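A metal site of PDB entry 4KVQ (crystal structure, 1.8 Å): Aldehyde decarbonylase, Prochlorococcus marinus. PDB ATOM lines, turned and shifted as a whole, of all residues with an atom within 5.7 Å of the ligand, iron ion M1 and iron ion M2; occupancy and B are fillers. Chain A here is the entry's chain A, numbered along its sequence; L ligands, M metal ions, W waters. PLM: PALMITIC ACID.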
ATOM      1  N   TYR A  35      -9.509  -5.459  30.156  1.00  0.00           N
ATOM      2  CA  TYR A  35      -8.085  -5.245  29.857  1.00  0.00           C
ATOM      3  C   TYR A  35      -7.316  -6.553  29.991  1.00  0.00           C
ATOM      4  O   TYR A  35      -6.348  -6.767  29.268  1.00  0.00           O
ATOM      5  CB  TYR A  35      -7.490  -4.162  30.761  1.00  0.00           C
ATOM      6  CG  TYR A  35      -6.277  -3.456  30.139  1.00  0.00           C
ATOM      7  CD1 TYR A  35      -6.442  -2.411  29.246  1.00  0.00           C
ATOM      8  CD2 TYR A  35      -4.975  -3.855  30.447  1.00  0.00           C
ATOM      9  CE1 TYR A  35      -5.346  -1.774  28.661  1.00  0.00           C
ATOM     10  CE2 TYR A  35      -3.874  -3.216  29.884  1.00  0.00           C
ATOM     11  CZ  TYR A  35      -4.070  -2.179  28.989  1.00  0.00           C
ATOM     12  OH  TYR A  35      -2.990  -1.534  28.425  1.00  0.00           O
ATOM     13  N   ILE A  38      -7.738  -8.104  26.521  1.00  0.00           N
ATOM     14  CA  ILE A  38      -7.150  -7.287  25.450  1.00  0.00           C
ATOM     15  C   ILE A  38      -5.618  -7.231  25.573  1.00  0.00           C
ATOM     16  O   ILE A  38      -4.893  -7.394  24.588  1.00  0.00           O
ATOM     17  CB  ILE A  38      -7.688  -5.858  25.491  1.00  0.00           C
ATOM     18  CG1 ILE A  38      -9.177  -5.846  25.185  1.00  0.00           C
ATOM     19  CG2 ILE A  38      -6.940  -4.944  24.490  1.00  0.00           C
ATOM     20  CD1 ILE A  38      -9.488  -6.416  23.871  1.00  0.00           C
ATOM     21  N   ILE A  41      -4.148 -10.535  24.484  1.00  0.00           N
ATOM     22  CA  ILE A  41      -4.154 -10.677  23.029  1.00  0.00           C
ATOM     23  C   ILE A  41      -2.992  -9.921  22.393  1.00  0.00           C
ATOM     24  O   ILE A  41      -2.319 -10.456  21.513  1.00  0.00           O
ATOM     25  CB  ILE A  41      -5.513 -10.193  22.434  1.00  0.00           C
ATOM     26  CG1 ILE A  41      -6.595 -11.237  22.717  1.00  0.00           C
ATOM     27  CG2 ILE A  41      -5.402  -9.958  20.934  1.00  0.00           C
ATOM     28  CD1 ILE A  41      -8.007 -10.772  22.370  1.00  0.00           C
ATOM     29  N   VAL A  42      -2.743  -8.708  22.856  1.00  0.00           N
ATOM     30  CA  VAL A  42      -1.623  -7.928  22.319  1.00  0.00           C
ATOM     31  C   VAL A  42      -0.271  -8.604  22.642  1.00  0.00           C
ATOM     32  O   VAL A  42       0.591  -8.727  21.780  1.00  0.00           O
ATOM     33  CB  VAL A  42      -1.675  -6.471  22.823  1.00  0.00           C
ATOM     34  CG1 VAL A  42      -0.455  -5.735  22.385  1.00  0.00           C
ATOM     35  CG2 VAL A  42      -2.935  -5.767  22.288  1.00  0.00           C
ATOM     36  N   GLY A  45       0.056 -11.601  20.490  1.00  0.00           N
ATOM     37  CA  GLY A  45       0.237 -11.210  19.118  1.00  0.00           C
ATOM     38  C   GLY A  45       1.668 -10.780  18.835  1.00  0.00           C
ATOM     39  O   GLY A  45       2.207 -11.091  17.768  1.00  0.00           O
ATOM     40  N   GLU A  46       2.259 -10.037  19.755  1.00  0.00           N
ATOM     41  CA  GLU A  46       3.649  -9.606  19.609  1.00  0.00           C
ATOM     42  C   GLU A  46       4.593 -10.794  19.627  1.00  0.00           C
ATOM     43  O   GLU A  46       5.543 -10.841  18.871  1.00  0.00           O
ATOM     44  CB  GLU A  46       4.029  -8.599  20.702  1.00  0.00           C
ATOM     45  CG  GLU A  46       3.181  -7.329  20.699  1.00  0.00           C
ATOM     46  CD  GLU A  46       3.461  -6.432  19.502  1.00  0.00           C
ATOM     47  OE1 GLU A  46       4.434  -6.715  18.762  1.00  0.00           O
ATOM     48  OE2 GLU A  46       2.717  -5.448  19.297  1.00  0.00           O
ATOM     49  N   ALA A  49       4.220 -12.473  16.340  1.00  0.00           N
ATOM     50  CA  ALA A  49       4.892 -11.686  15.301  1.00  0.00           C
ATOM     51  C   ALA A  49       6.386 -12.003  15.323  1.00  0.00           C
ATOM     52  O   ALA A  49       6.994 -12.247  14.276  1.00  0.00           O
ATOM     53  CB  ALA A  49       4.628 -10.186  15.496  1.00  0.00           C
ATOM     54  N   TYR A  53       8.325 -13.763  12.062  1.00  0.00           N
ATOM     55  CA  TYR A  53       9.431 -13.193  11.303  1.00  0.00           C
ATOM     56  C   TYR A  53      10.658 -14.118  11.350  1.00  0.00           C
ATOM     57  O   TYR A  53      11.338 -14.280  10.347  1.00  0.00           O
ATOM     58  CB  TYR A  53       9.775 -11.767  11.757  1.00  0.00           C
ATOM     59  CG  TYR A  53       8.736 -10.769  11.311  1.00  0.00           C
ATOM     60  CD1 TYR A  53       8.426 -10.616   9.962  1.00  0.00           C
ATOM     61  CD2 TYR A  53       8.048  -9.975  12.231  1.00  0.00           C
ATOM     62  CE1 TYR A  53       7.465  -9.705   9.536  1.00  0.00           C
ATOM     63  CE2 TYR A  53       7.085  -9.056  11.800  1.00  0.00           C
ATOM     64  CZ  TYR A  53       6.802  -8.939  10.458  1.00  0.00           C
ATOM     65  OH  TYR A  53       5.843  -8.036  10.037  1.00  0.00           O
ATOM     66  N   MET A  73      12.290  -6.238  17.483  1.00  0.00           N
ATOM     67  CA  MET A  73      11.352  -5.154  17.747  1.00  0.00           C
ATOM     68  C   MET A  73      10.078  -5.704  18.374  1.00  0.00           C
ATOM     69  O   MET A  73       9.517  -5.097  19.287  1.00  0.00           O
ATOM     70  CB  MET A  73      10.988  -4.368  16.475  1.00  0.00           C
ATOM     71  CG  MET A  73      12.143  -3.663  15.778  1.00  0.00           C
ATOM     72  SD  MET A  73      11.554  -2.768  14.312  1.00  0.00           S
ATOM     73  CE  MET A  73      13.121  -2.458  13.474  1.00  0.00           C
ATOM     74  N   GLU A  74       9.610  -6.841  17.858  1.00  0.00           N
ATOM     75  CA  GLU A  74       8.378  -7.441  18.367  1.00  0.00           C
ATOM     76  C   GLU A  74       8.547  -7.814  19.832  1.00  0.00           C
ATOM     77  O   GLU A  74       7.615  -7.679  20.625  1.00  0.00           O
ATOM     78  CB  GLU A  74       7.952  -8.660  17.538  1.00  0.00           C
ATOM     79  CG  GLU A  74       7.774  -8.378  16.026  1.00  0.00           C
ATOM     80  CD  GLU A  74       6.657  -7.383  15.689  1.00  0.00           C
ATOM     81  OE1 GLU A  74       6.230  -6.609  16.559  1.00  0.00           O
ATOM     82  OE2 GLU A  74       6.219  -7.362  14.515  1.00  0.00           O
ATOM     83  N   HIS A  77       8.105  -4.721  21.855  1.00  0.00           N
ATOM     84  CA  HIS A  77       6.670  -4.395  21.962  1.00  0.00           C
ATOM     85  C   HIS A  77       6.016  -5.280  23.027  1.00  0.00           C
ATOM     86  O   HIS A  77       5.234  -4.813  23.847  1.00  0.00           O
ATOM     87  CB  HIS A  77       5.958  -4.632  20.623  1.00  0.00           C
ATOM     88  CG  HIS A  77       6.535  -3.864  19.477  1.00  0.00           C
ATOM     89  ND1 HIS A  77       6.162  -4.098  18.171  1.00  0.00           N
ATOM     90  CD2 HIS A  77       7.439  -2.853  19.435  1.00  0.00           C
ATOM     91  CE1 HIS A  77       6.822  -3.281  17.366  1.00  0.00           C
ATOM     92  NE2 HIS A  77       7.608  -2.518  18.113  1.00  0.00           N
ATOM     93  N   PHE A  81       4.031  -3.945  26.342  1.00  0.00           N
ATOM     94  CA  PHE A  81       2.617  -4.196  26.616  1.00  0.00           C
ATOM     95  C   PHE A  81       2.434  -5.052  27.857  1.00  0.00           C
ATOM     96  O   PHE A  81       1.456  -4.912  28.581  1.00  0.00           O
ATOM     97  CB  PHE A  81       1.945  -4.805  25.379  1.00  0.00           C
ATOM     98  CG  PHE A  81       1.776  -3.833  24.247  1.00  0.00           C
ATOM     99  CD1 PHE A  81       1.164  -2.608  24.480  1.00  0.00           C
ATOM    100  CD2 PHE A  81       2.233  -4.109  22.978  1.00  0.00           C
ATOM    101  CE1 PHE A  81       1.002  -1.682  23.448  1.00  0.00           C
ATOM    102  CE2 PHE A  81       2.059  -3.195  21.932  1.00  0.00           C
ATOM    103  CZ  PHE A  81       1.452  -1.986  22.174  1.00  0.00           C
ATOM    104  N   PHE A 100      -7.557 -17.129  20.743  1.00  0.00           N
ATOM    105  CA  PHE A 100      -7.900 -16.039  19.823  1.00  0.00           C
ATOM    106  C   PHE A 100      -7.069 -16.096  18.550  1.00  0.00           C
ATOM    107  O   PHE A 100      -7.597 -15.882  17.457  1.00  0.00           O
ATOM    108  CB  PHE A 100      -7.668 -14.707  20.547  1.00  0.00           C
ATOM    109  CG  PHE A 100      -8.002 -13.484  19.744  1.00  0.00           C
ATOM    110  CD1 PHE A 100      -9.318 -13.036  19.623  1.00  0.00           C
ATOM    111  CD2 PHE A 100      -6.993 -12.724  19.164  1.00  0.00           C
ATOM    112  CE1 PHE A 100      -9.609 -11.885  18.920  1.00  0.00           C
ATOM    113  CE2 PHE A 100      -7.283 -11.572  18.461  1.00  0.00           C
ATOM    114  CZ  PHE A 100      -8.596 -11.141  18.350  1.00  0.00           C
ATOM    115  N   PHE A 101      -5.771 -16.354  18.695  1.00  0.00           N
ATOM    116  CA  PHE A 101      -4.835 -16.402  17.569  1.00  0.00           C
ATOM    117  C   PHE A 101      -4.723 -17.761  16.884  1.00  0.00           C
ATOM    118  O   PHE A 101      -4.132 -17.847  15.809  1.00  0.00           O
ATOM    119  CB  PHE A 101      -3.441 -15.947  17.995  1.00  0.00           C
ATOM    120  CG  PHE A 101      -3.291 -14.464  17.997  1.00  0.00           C
ATOM    121  CD1 PHE A 101      -3.136 -13.790  16.806  1.00  0.00           C
ATOM    122  CD2 PHE A 101      -3.329 -13.743  19.180  1.00  0.00           C
ATOM    123  CE1 PHE A 101      -3.018 -12.408  16.794  1.00  0.00           C
ATOM    124  CE2 PHE A 101      -3.222 -12.368  19.162  1.00  0.00           C
ATOM    125  CZ  PHE A 101      -3.065 -11.702  17.976  1.00  0.00           C
ATOM    126  N   GLN A 124       1.351 -12.264   8.139  1.00  0.00           N
ATOM    127  CA  GLN A 124       1.994 -11.506   9.199  1.00  0.00           C
ATOM    128  C   GLN A 124       2.207 -10.048   8.836  1.00  0.00           C
ATOM    129  O   GLN A 124       1.763  -9.161   9.563  1.00  0.00           O
ATOM    130  CB  GLN A 124       3.345 -12.107   9.606  1.00  0.00           C
ATOM    131  CG  GLN A 124       4.120 -11.173  10.580  1.00  0.00           C
ATOM    132  CD  GLN A 124       3.398 -10.934  11.888  1.00  0.00           C
ATOM    133  OE1 GLN A 124       2.861 -11.862  12.495  1.00  0.00           O
ATOM    134  NE2 GLN A 124       3.379  -9.666  12.342  1.00  0.00           N
ATOM    135  N   ILE A 128      -1.811  -9.002   9.851  1.00  0.00           N
ATOM    136  CA  ILE A 128      -1.600  -8.809  11.279  1.00  0.00           C
ATOM    137  C   ILE A 128      -1.015  -7.432  11.586  1.00  0.00           C
ATOM    138  O   ILE A 128      -1.463  -6.778  12.525  1.00  0.00           O
ATOM    139  CB  ILE A 128      -0.782  -9.952  11.900  1.00  0.00           C
ATOM    140  CG1 ILE A 128      -1.576 -11.257  11.805  1.00  0.00           C
ATOM    141  CG2 ILE A 128      -0.467  -9.647  13.348  1.00  0.00           C
ATOM    142  CD1 ILE A 128      -0.843 -12.471  12.327  1.00  0.00           C
ATOM    143  N   GLU A 129      -0.062  -6.951  10.788  1.00  0.00           N
ATOM    144  CA  GLU A 129       0.473  -5.614  11.032  1.00  0.00           C
ATOM    145  C   GLU A 129      -0.609  -4.542  10.844  1.00  0.00           C
ATOM    146  O   GLU A 129      -0.700  -3.624  11.644  1.00  0.00           O
ATOM    147  CB  GLU A 129       1.673  -5.276  10.145  1.00  0.00           C
ATOM    148  CG  GLU A 129       2.883  -6.186  10.305  1.00  0.00           C
ATOM    149  CD  GLU A 129       3.606  -6.042  11.643  1.00  0.00           C
ATOM    150  OE1 GLU A 129       3.370  -5.056  12.383  1.00  0.00           O
ATOM    151  OE2 GLU A 129       4.464  -6.919  11.953  1.00  0.00           O
ATOM    152  N   PHE A 131      -3.829  -4.939  11.284  1.00  0.00           N
ATOM    153  CA  PHE A 131      -4.748  -5.102  12.412  1.00  0.00           C
ATOM    154  C   PHE A 131      -4.152  -4.396  13.645  1.00  0.00           C
ATOM    155  O   PHE A 131      -4.832  -3.651  14.342  1.00  0.00           O
ATOM    156  CB  PHE A 131      -4.951  -6.604  12.659  1.00  0.00           C
ATOM    157  CG  PHE A 131      -5.992  -6.937  13.699  1.00  0.00           C
ATOM    158  CD1 PHE A 131      -6.918  -5.998  14.114  1.00  0.00           C
ATOM    159  CD2 PHE A 131      -6.030  -8.203  14.260  1.00  0.00           C
ATOM    160  CE1 PHE A 131      -7.876  -6.320  15.075  1.00  0.00           C
ATOM    161  CE2 PHE A 131      -6.975  -8.533  15.224  1.00  0.00           C
ATOM    162  CZ  PHE A 131      -7.894  -7.584  15.632  1.00  0.00           C
ATOM    163  N   ALA A 132      -2.860  -4.616  13.874  1.00  0.00           N
ATOM    164  CA  ALA A 132      -2.168  -3.978  14.992  1.00  0.00           C
ATOM    165  C   ALA A 132      -2.164  -2.463  14.875  1.00  0.00           C
ATOM    166  O   ALA A 132      -2.460  -1.758  15.830  1.00  0.00           O
ATOM    167  CB  ALA A 132      -0.736  -4.484  15.086  1.00  0.00           C
ATOM    168  N   ALA A 135      -5.581  -1.093  15.544  1.00  0.00           N
ATOM    169  CA  ALA A 135      -5.907  -1.244  16.962  1.00  0.00           C
ATOM    170  C   ALA A 135      -5.126  -0.251  17.813  1.00  0.00           C
ATOM    171  O   ALA A 135      -5.697   0.419  18.675  1.00  0.00           O
ATOM    172  CB  ALA A 135      -5.623  -2.653  17.401  1.00  0.00           C
ATOM    173  N   TYR A 136      -3.828  -0.155  17.573  1.00  0.00           N
ATOM    174  CA  TYR A 136      -3.019   0.765  18.371  1.00  0.00           C
ATOM    175  C   TYR A 136      -3.412   2.222  18.157  1.00  0.00           C
ATOM    176  O   TYR A 136      -3.488   2.987  19.113  1.00  0.00           O
ATOM    177  CB  TYR A 136      -1.521   0.534  18.097  1.00  0.00           C
ATOM    178  CG  TYR A 136      -1.040  -0.857  18.460  1.00  0.00           C
ATOM    179  CD1 TYR A 136      -1.771  -1.677  19.313  1.00  0.00           C
ATOM    180  CD2 TYR A 136       0.143  -1.356  17.925  1.00  0.00           C
ATOM    181  CE1 TYR A 136      -1.334  -2.960  19.636  1.00  0.00           C
ATOM    182  CE2 TYR A 136       0.591  -2.651  18.242  1.00  0.00           C
ATOM    183  CZ  TYR A 136      -0.157  -3.428  19.094  1.00  0.00           C
ATOM    184  OH  TYR A 136       0.275  -4.700  19.399  1.00  0.00           O
ATOM    185  N   TYR A 139      -6.593   2.828  20.091  1.00  0.00           N
ATOM    186  CA  TYR A 139      -6.398   2.775  21.537  1.00  0.00           C
ATOM    187  C   TYR A 139      -5.717   4.019  22.096  1.00  0.00           C
ATOM    188  O   TYR A 139      -6.036   4.447  23.198  1.00  0.00           O
ATOM    189  CB  TYR A 139      -5.578   1.537  21.883  1.00  0.00           C
ATOM    190  CG  TYR A 139      -5.125   1.395  23.325  1.00  0.00           C
ATOM    191  CD1 TYR A 139      -6.041   1.303  24.370  1.00  0.00           C
ATOM    192  CD2 TYR A 139      -3.762   1.255  23.636  1.00  0.00           C
ATOM    193  CE1 TYR A 139      -5.623   1.131  25.681  1.00  0.00           C
ATOM    194  CE2 TYR A 139      -3.343   1.075  24.951  1.00  0.00           C
ATOM    195  CZ  TYR A 139      -4.271   1.019  25.963  1.00  0.00           C
ATOM    196  OH  TYR A 139      -3.846   0.844  27.263  1.00  0.00           O
ATOM    197  N   THR A 151       2.478   2.672  23.593  1.00  0.00           N
ATOM    198  CA  THR A 151       1.808   2.412  22.336  1.00  0.00           C
ATOM    199  C   THR A 151       2.245   3.366  21.222  1.00  0.00           C
ATOM    200  O   THR A 151       2.395   2.959  20.071  1.00  0.00           O
ATOM    201  CB  THR A 151       0.267   2.455  22.497  1.00  0.00           C
ATOM    202  OG1 THR A 151      -0.123   1.659  23.634  1.00  0.00           O
ATOM    203  CG2 THR A 151      -0.417   1.915  21.242  1.00  0.00           C
ATOM    204  N   VAL A 154       5.416   2.040  19.828  1.00  0.00           N
ATOM    205  CA  VAL A 154       5.247   0.817  19.036  1.00  0.00           C
ATOM    206  C   VAL A 154       4.732   1.079  17.621  1.00  0.00           C
ATOM    207  O   VAL A 154       5.175   0.436  16.664  1.00  0.00           O
ATOM    208  CB  VAL A 154       4.291  -0.164  19.763  1.00  0.00           C
ATOM    209  CG1 VAL A 154       3.772  -1.227  18.799  1.00  0.00           C
ATOM    210  CG2 VAL A 154       4.993  -0.820  20.961  1.00  0.00           C
ATOM    211  N   ASP A 157       7.088   1.428  14.662  1.00  0.00           N
ATOM    212  CA  ASP A 157       7.719   0.185  14.234  1.00  0.00           C
ATOM    213  C   ASP A 157       6.822  -0.608  13.307  1.00  0.00           C
ATOM    214  O   ASP A 157       7.309  -1.286  12.390  1.00  0.00           O
ATOM    215  CB  ASP A 157       8.078  -0.712  15.423  1.00  0.00           C
ATOM    216  CG  ASP A 157       9.307  -0.238  16.172  1.00  0.00           C
ATOM    217  OD1 ASP A 157      10.011   0.654  15.647  1.00  0.00           O
ATOM    218  OD2 ASP A 157       9.566  -0.777  17.263  1.00  0.00           O
ATOM    219  N   GLU A 158       5.515  -0.571  13.534  1.00  0.00           N
ATOM    220  CA  GLU A 158       4.651  -1.453  12.743  1.00  0.00           C
ATOM    221  C   GLU A 158       4.570  -0.957  11.282  1.00  0.00           C
ATOM    222  O   GLU A 158       4.380  -1.759  10.364  1.00  0.00           O
ATOM    223  CB  GLU A 158       3.271  -1.690  13.399  1.00  0.00           C
ATOM    224  CG  GLU A 158       3.291  -1.951  14.957  1.00  0.00           C
ATOM    225  CD  GLU A 158       3.874  -3.311  15.464  1.00  0.00           C
ATOM    226  OE1 GLU A 158       3.475  -3.727  16.596  1.00  0.00           O
ATOM    227  OE2 GLU A 158       4.727  -3.964  14.802  1.00  0.00           O
ATOM    228  N   HIS A 161       7.262  -2.588   9.519  1.00  0.00           N
ATOM    229  CA  HIS A 161       7.014  -3.997   9.267  1.00  0.00           C
ATOM    230  C   HIS A 161       6.141  -4.149   8.041  1.00  0.00           C
ATOM    231  O   HIS A 161       6.403  -4.988   7.178  1.00  0.00           O
ATOM    232  CB  HIS A 161       6.368  -4.632  10.505  1.00  0.00           C
ATOM    233  CG  HIS A 161       7.244  -4.607  11.717  1.00  0.00           C
ATOM    234  ND1 HIS A 161       6.805  -5.007  12.953  1.00  0.00           N
ATOM    235  CD2 HIS A 161       8.523  -4.228  11.873  1.00  0.00           C
ATOM    236  CE1 HIS A 161       7.785  -4.873  13.826  1.00  0.00           C
ATOM    237  NE2 HIS A 161       8.849  -4.394  13.193  1.00  0.00           N
ATOM    238  N   VAL A 198     -13.208  -9.338  19.550  1.00  0.00           N
ATOM    239  CA  VAL A 198     -12.559  -8.385  20.434  1.00  0.00           C
ATOM    240  C   VAL A 198     -13.455  -7.174  20.730  1.00  0.00           C
ATOM    241  O   VAL A 198     -13.211  -6.412  21.677  1.00  0.00           O
ATOM    242  CB  VAL A 198     -11.204  -7.962  19.818  1.00  0.00           C
ATOM    243  CG1 VAL A 198     -11.329  -6.671  19.013  1.00  0.00           C
ATOM    244  CG2 VAL A 198     -10.138  -7.849  20.873  1.00  0.00           C
ATOM    245  N   ALA A 202     -13.135  -4.347  23.618  1.00  0.00           N
ATOM    246  CA  ALA A 202     -12.649  -3.081  23.075  1.00  0.00           C
ATOM    247  C   ALA A 202     -13.576  -1.929  23.425  1.00  0.00           C
ATOM    248  O   ALA A 202     -13.109  -0.822  23.696  1.00  0.00           O
ATOM    249  CB  ALA A 202     -12.431  -3.173  21.542  1.00  0.00           C
ATOM    250  N   LEU A 205     -13.013  -0.580  26.718  1.00  0.00           N
ATOM    251  CA  LEU A 205     -11.825   0.262  26.647  1.00  0.00           C
ATOM    252  C   LEU A 205     -12.073   1.585  25.911  1.00  0.00           C
ATOM    253  O   LEU A 205     -11.134   2.343  25.655  1.00  0.00           O
ATOM    254  CB  LEU A 205     -10.665  -0.503  26.000  1.00  0.00           C
ATOM    255  CG  LEU A 205      -9.729  -1.301  26.920  1.00  0.00           C
ATOM    256  CD1 LEU A 205     -10.458  -2.339  27.747  1.00  0.00           C
ATOM    257  CD2 LEU A 205      -8.656  -1.981  26.075  1.00  0.00           C
ATOM    258  N   MET A 207     -13.136   1.960  22.811  1.00  0.00           N
ATOM    259  CA  MET A 207     -12.778   1.885  21.403  1.00  0.00           C
ATOM    260  C   MET A 207     -14.003   1.481  20.571  1.00  0.00           C
ATOM    261  O   MET A 207     -14.680   0.519  20.909  1.00  0.00           O
ATOM    262  CB  MET A 207     -11.664   0.861  21.219  1.00  0.00           C
ATOM    263  CG  MET A 207     -10.372   1.245  21.969  1.00  0.00           C
ATOM    264  SD  MET A 207      -9.180  -0.121  22.019  1.00  0.00           S
ATOM    265  CE  MET A 207      -8.778  -0.200  20.307  1.00  0.00           C
ATOM    266  N   LEU A 212     -12.085   0.597  14.394  1.00  0.00           N
ATOM    267  CA  LEU A 212     -11.166  -0.531  14.245  1.00  0.00           C
ATOM    268  C   LEU A 212     -11.255  -1.129  12.846  1.00  0.00           C
ATOM    269  O   LEU A 212     -10.247  -1.378  12.187  1.00  0.00           O
ATOM    270  CB  LEU A 212     -11.447  -1.603  15.293  1.00  0.00           C
ATOM    271  CG  LEU A 212     -11.035  -1.334  16.738  1.00  0.00           C
ATOM    272  CD1 LEU A 212     -11.524  -2.446  17.674  1.00  0.00           C
ATOM    273  CD2 LEU A 212      -9.521  -1.206  16.830  1.00  0.00           C
HETATM  274  C1  PLM L   1       2.829  -7.027  15.346  1.00  0.00           C
HETATM  275  O1  PLM L   1       3.835  -6.366  15.552  1.00  0.00           O
HETATM  276  O2  PLM L   1       2.486  -7.617  14.290  1.00  0.00           O
HETATM  277  C2  PLM L   1       1.858  -7.118  16.556  1.00  0.00           C
HETATM  278  C3  PLM L   1       0.572  -7.874  16.297  1.00  0.00           C
HETATM  279  C4  PLM L   1      -0.415  -7.888  17.483  1.00  0.00           C
HETATM  280  C5  PLM L   1      -1.890  -7.850  17.074  1.00  0.00           C
HETATM  281  C6  PLM L   1      -2.788  -7.108  18.081  1.00  0.00           C
HETATM  282  C7  PLM L   1      -4.266  -7.009  17.694  1.00  0.00           C
HETATM  283  C8  PLM L   1      -5.207  -6.851  18.905  1.00  0.00           C
HETATM  284  C9  PLM L   1      -6.375  -5.895  18.685  1.00  0.00           C
HETATM  285  CA  PLM L   1      -7.272  -5.704  19.929  1.00  0.00           C
HETATM  286  CB  PLM L   1      -7.310  -4.259  20.487  1.00  0.00           C
HETATM  287  CC  PLM L   1      -6.011  -3.884  21.219  1.00  0.00           C
HETATM  288  CD  PLM L   1      -5.930  -2.423  21.630  1.00  0.00           C
HETATM  289  CE  PLM L   1      -4.501  -1.999  22.010  1.00  0.00           C
HETATM  290  CF  PLM L   1      -4.138  -2.289  23.465  1.00  0.00           C
HETATM  291  CG  PLM L   1      -2.646  -2.106  23.716  1.00  0.00           C
HETATM  292 FE    FE M   1       4.712  -5.421  17.152  1.00  0.00          FE
HETATM  293 FE    FE M   2       4.939  -5.889  13.833  1.00  0.00          FE
HETATM  294  O   HOH W   1      -2.035  -3.696  26.144  1.00  0.00           O
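NE2 of Gln 124 sits at hydrogen-bond distance from O2 of the ligand, 3.0 Å away.
OH of Tyr 136 is in hydrogen-bond range of OE2 of Glu 46, 2.6 Å away. The backbone NH (N) of Glu 129 lies within hydrogen-bond range of the backbone carbonyl oxygen (O) of Gln 124 (3.1 Å). OD2 of Asp 157 lies within hydrogen-bond range of NE2 of His 77. OH of Tyr 139 is in hydrogen-bond range of OH of Tyr 35 (2.8 Å). The side-chain hydroxyl of Tyr 53 lies close to the side-chain carboxylate of Glu 129 (2.6 Å). O of Met 73 sits close to NE2 of His 77 (3.4 Å). SD of Met 73 is in hydrogen-bond range of NE2 of His 161 (3.3 Å). The backbone NH of Met 207 is in hydrogen-bond range of the backbone carbonyl oxygen of Ala 202.
Merely in contact with the ligand: Ile 38, Ile 41, Val 42, Gly 45, Ala 49, Phe 81, Ile 128, Phe 131, Ala 132, Ala 135, Tyr 136, Tyr 139, Val 198 and Met 207. Hydrophobic or aromatic side chains within 4 Å of the ligand: Ile 38, Ile 41, Val 42, Ala 49, Phe 81, Ile 128, Phe 131, Ala 132, Ala 135, Tyr 136, Tyr 139, Val 198 and Met 207. 19 residues have an atom within 4 Å of the ligand: Ile 38, Ile 41, Val 42, Gly 45, Glu 46, Ala 49, Glu 74, Phe 81, Gln 124, Ile 128, Glu 129, Phe 131, Ala 132, Ala 135, Tyr 136, Tyr 139, Glu 158, Val 198 and Met 207.
Of the 32 residues printed, 4 come within 4 Å of iron ion M1.
Iron ion M1 is bound by the side-chain carboxylate of Glu 74 (2.0 Å), an oxygen (O1) of the ligand (2.1 Å), the side-chain carboxylate of Glu 46 (2.1 Å), the side-chain carboxylate of Glu 158 (2.2 Å) and a ring nitrogen (ND1) of His 77 (2.2 Å). Iron ion M1 has five donor atoms within binding distance. Slightly farther from iron ion M1 lies OE2 of Glu 158 (2.8 Å).
Iron ion M2 is bound by OE2 of Glu 74 (2.1 Å), O1 of the ligand (2.1 Å), OE2 of Glu 158 (2.2 Å), OE2 of Glu 129 (2.2 Å), ND1 of His 161 (2.2 Å) and OE1 of Glu 129 (2.3 Å).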
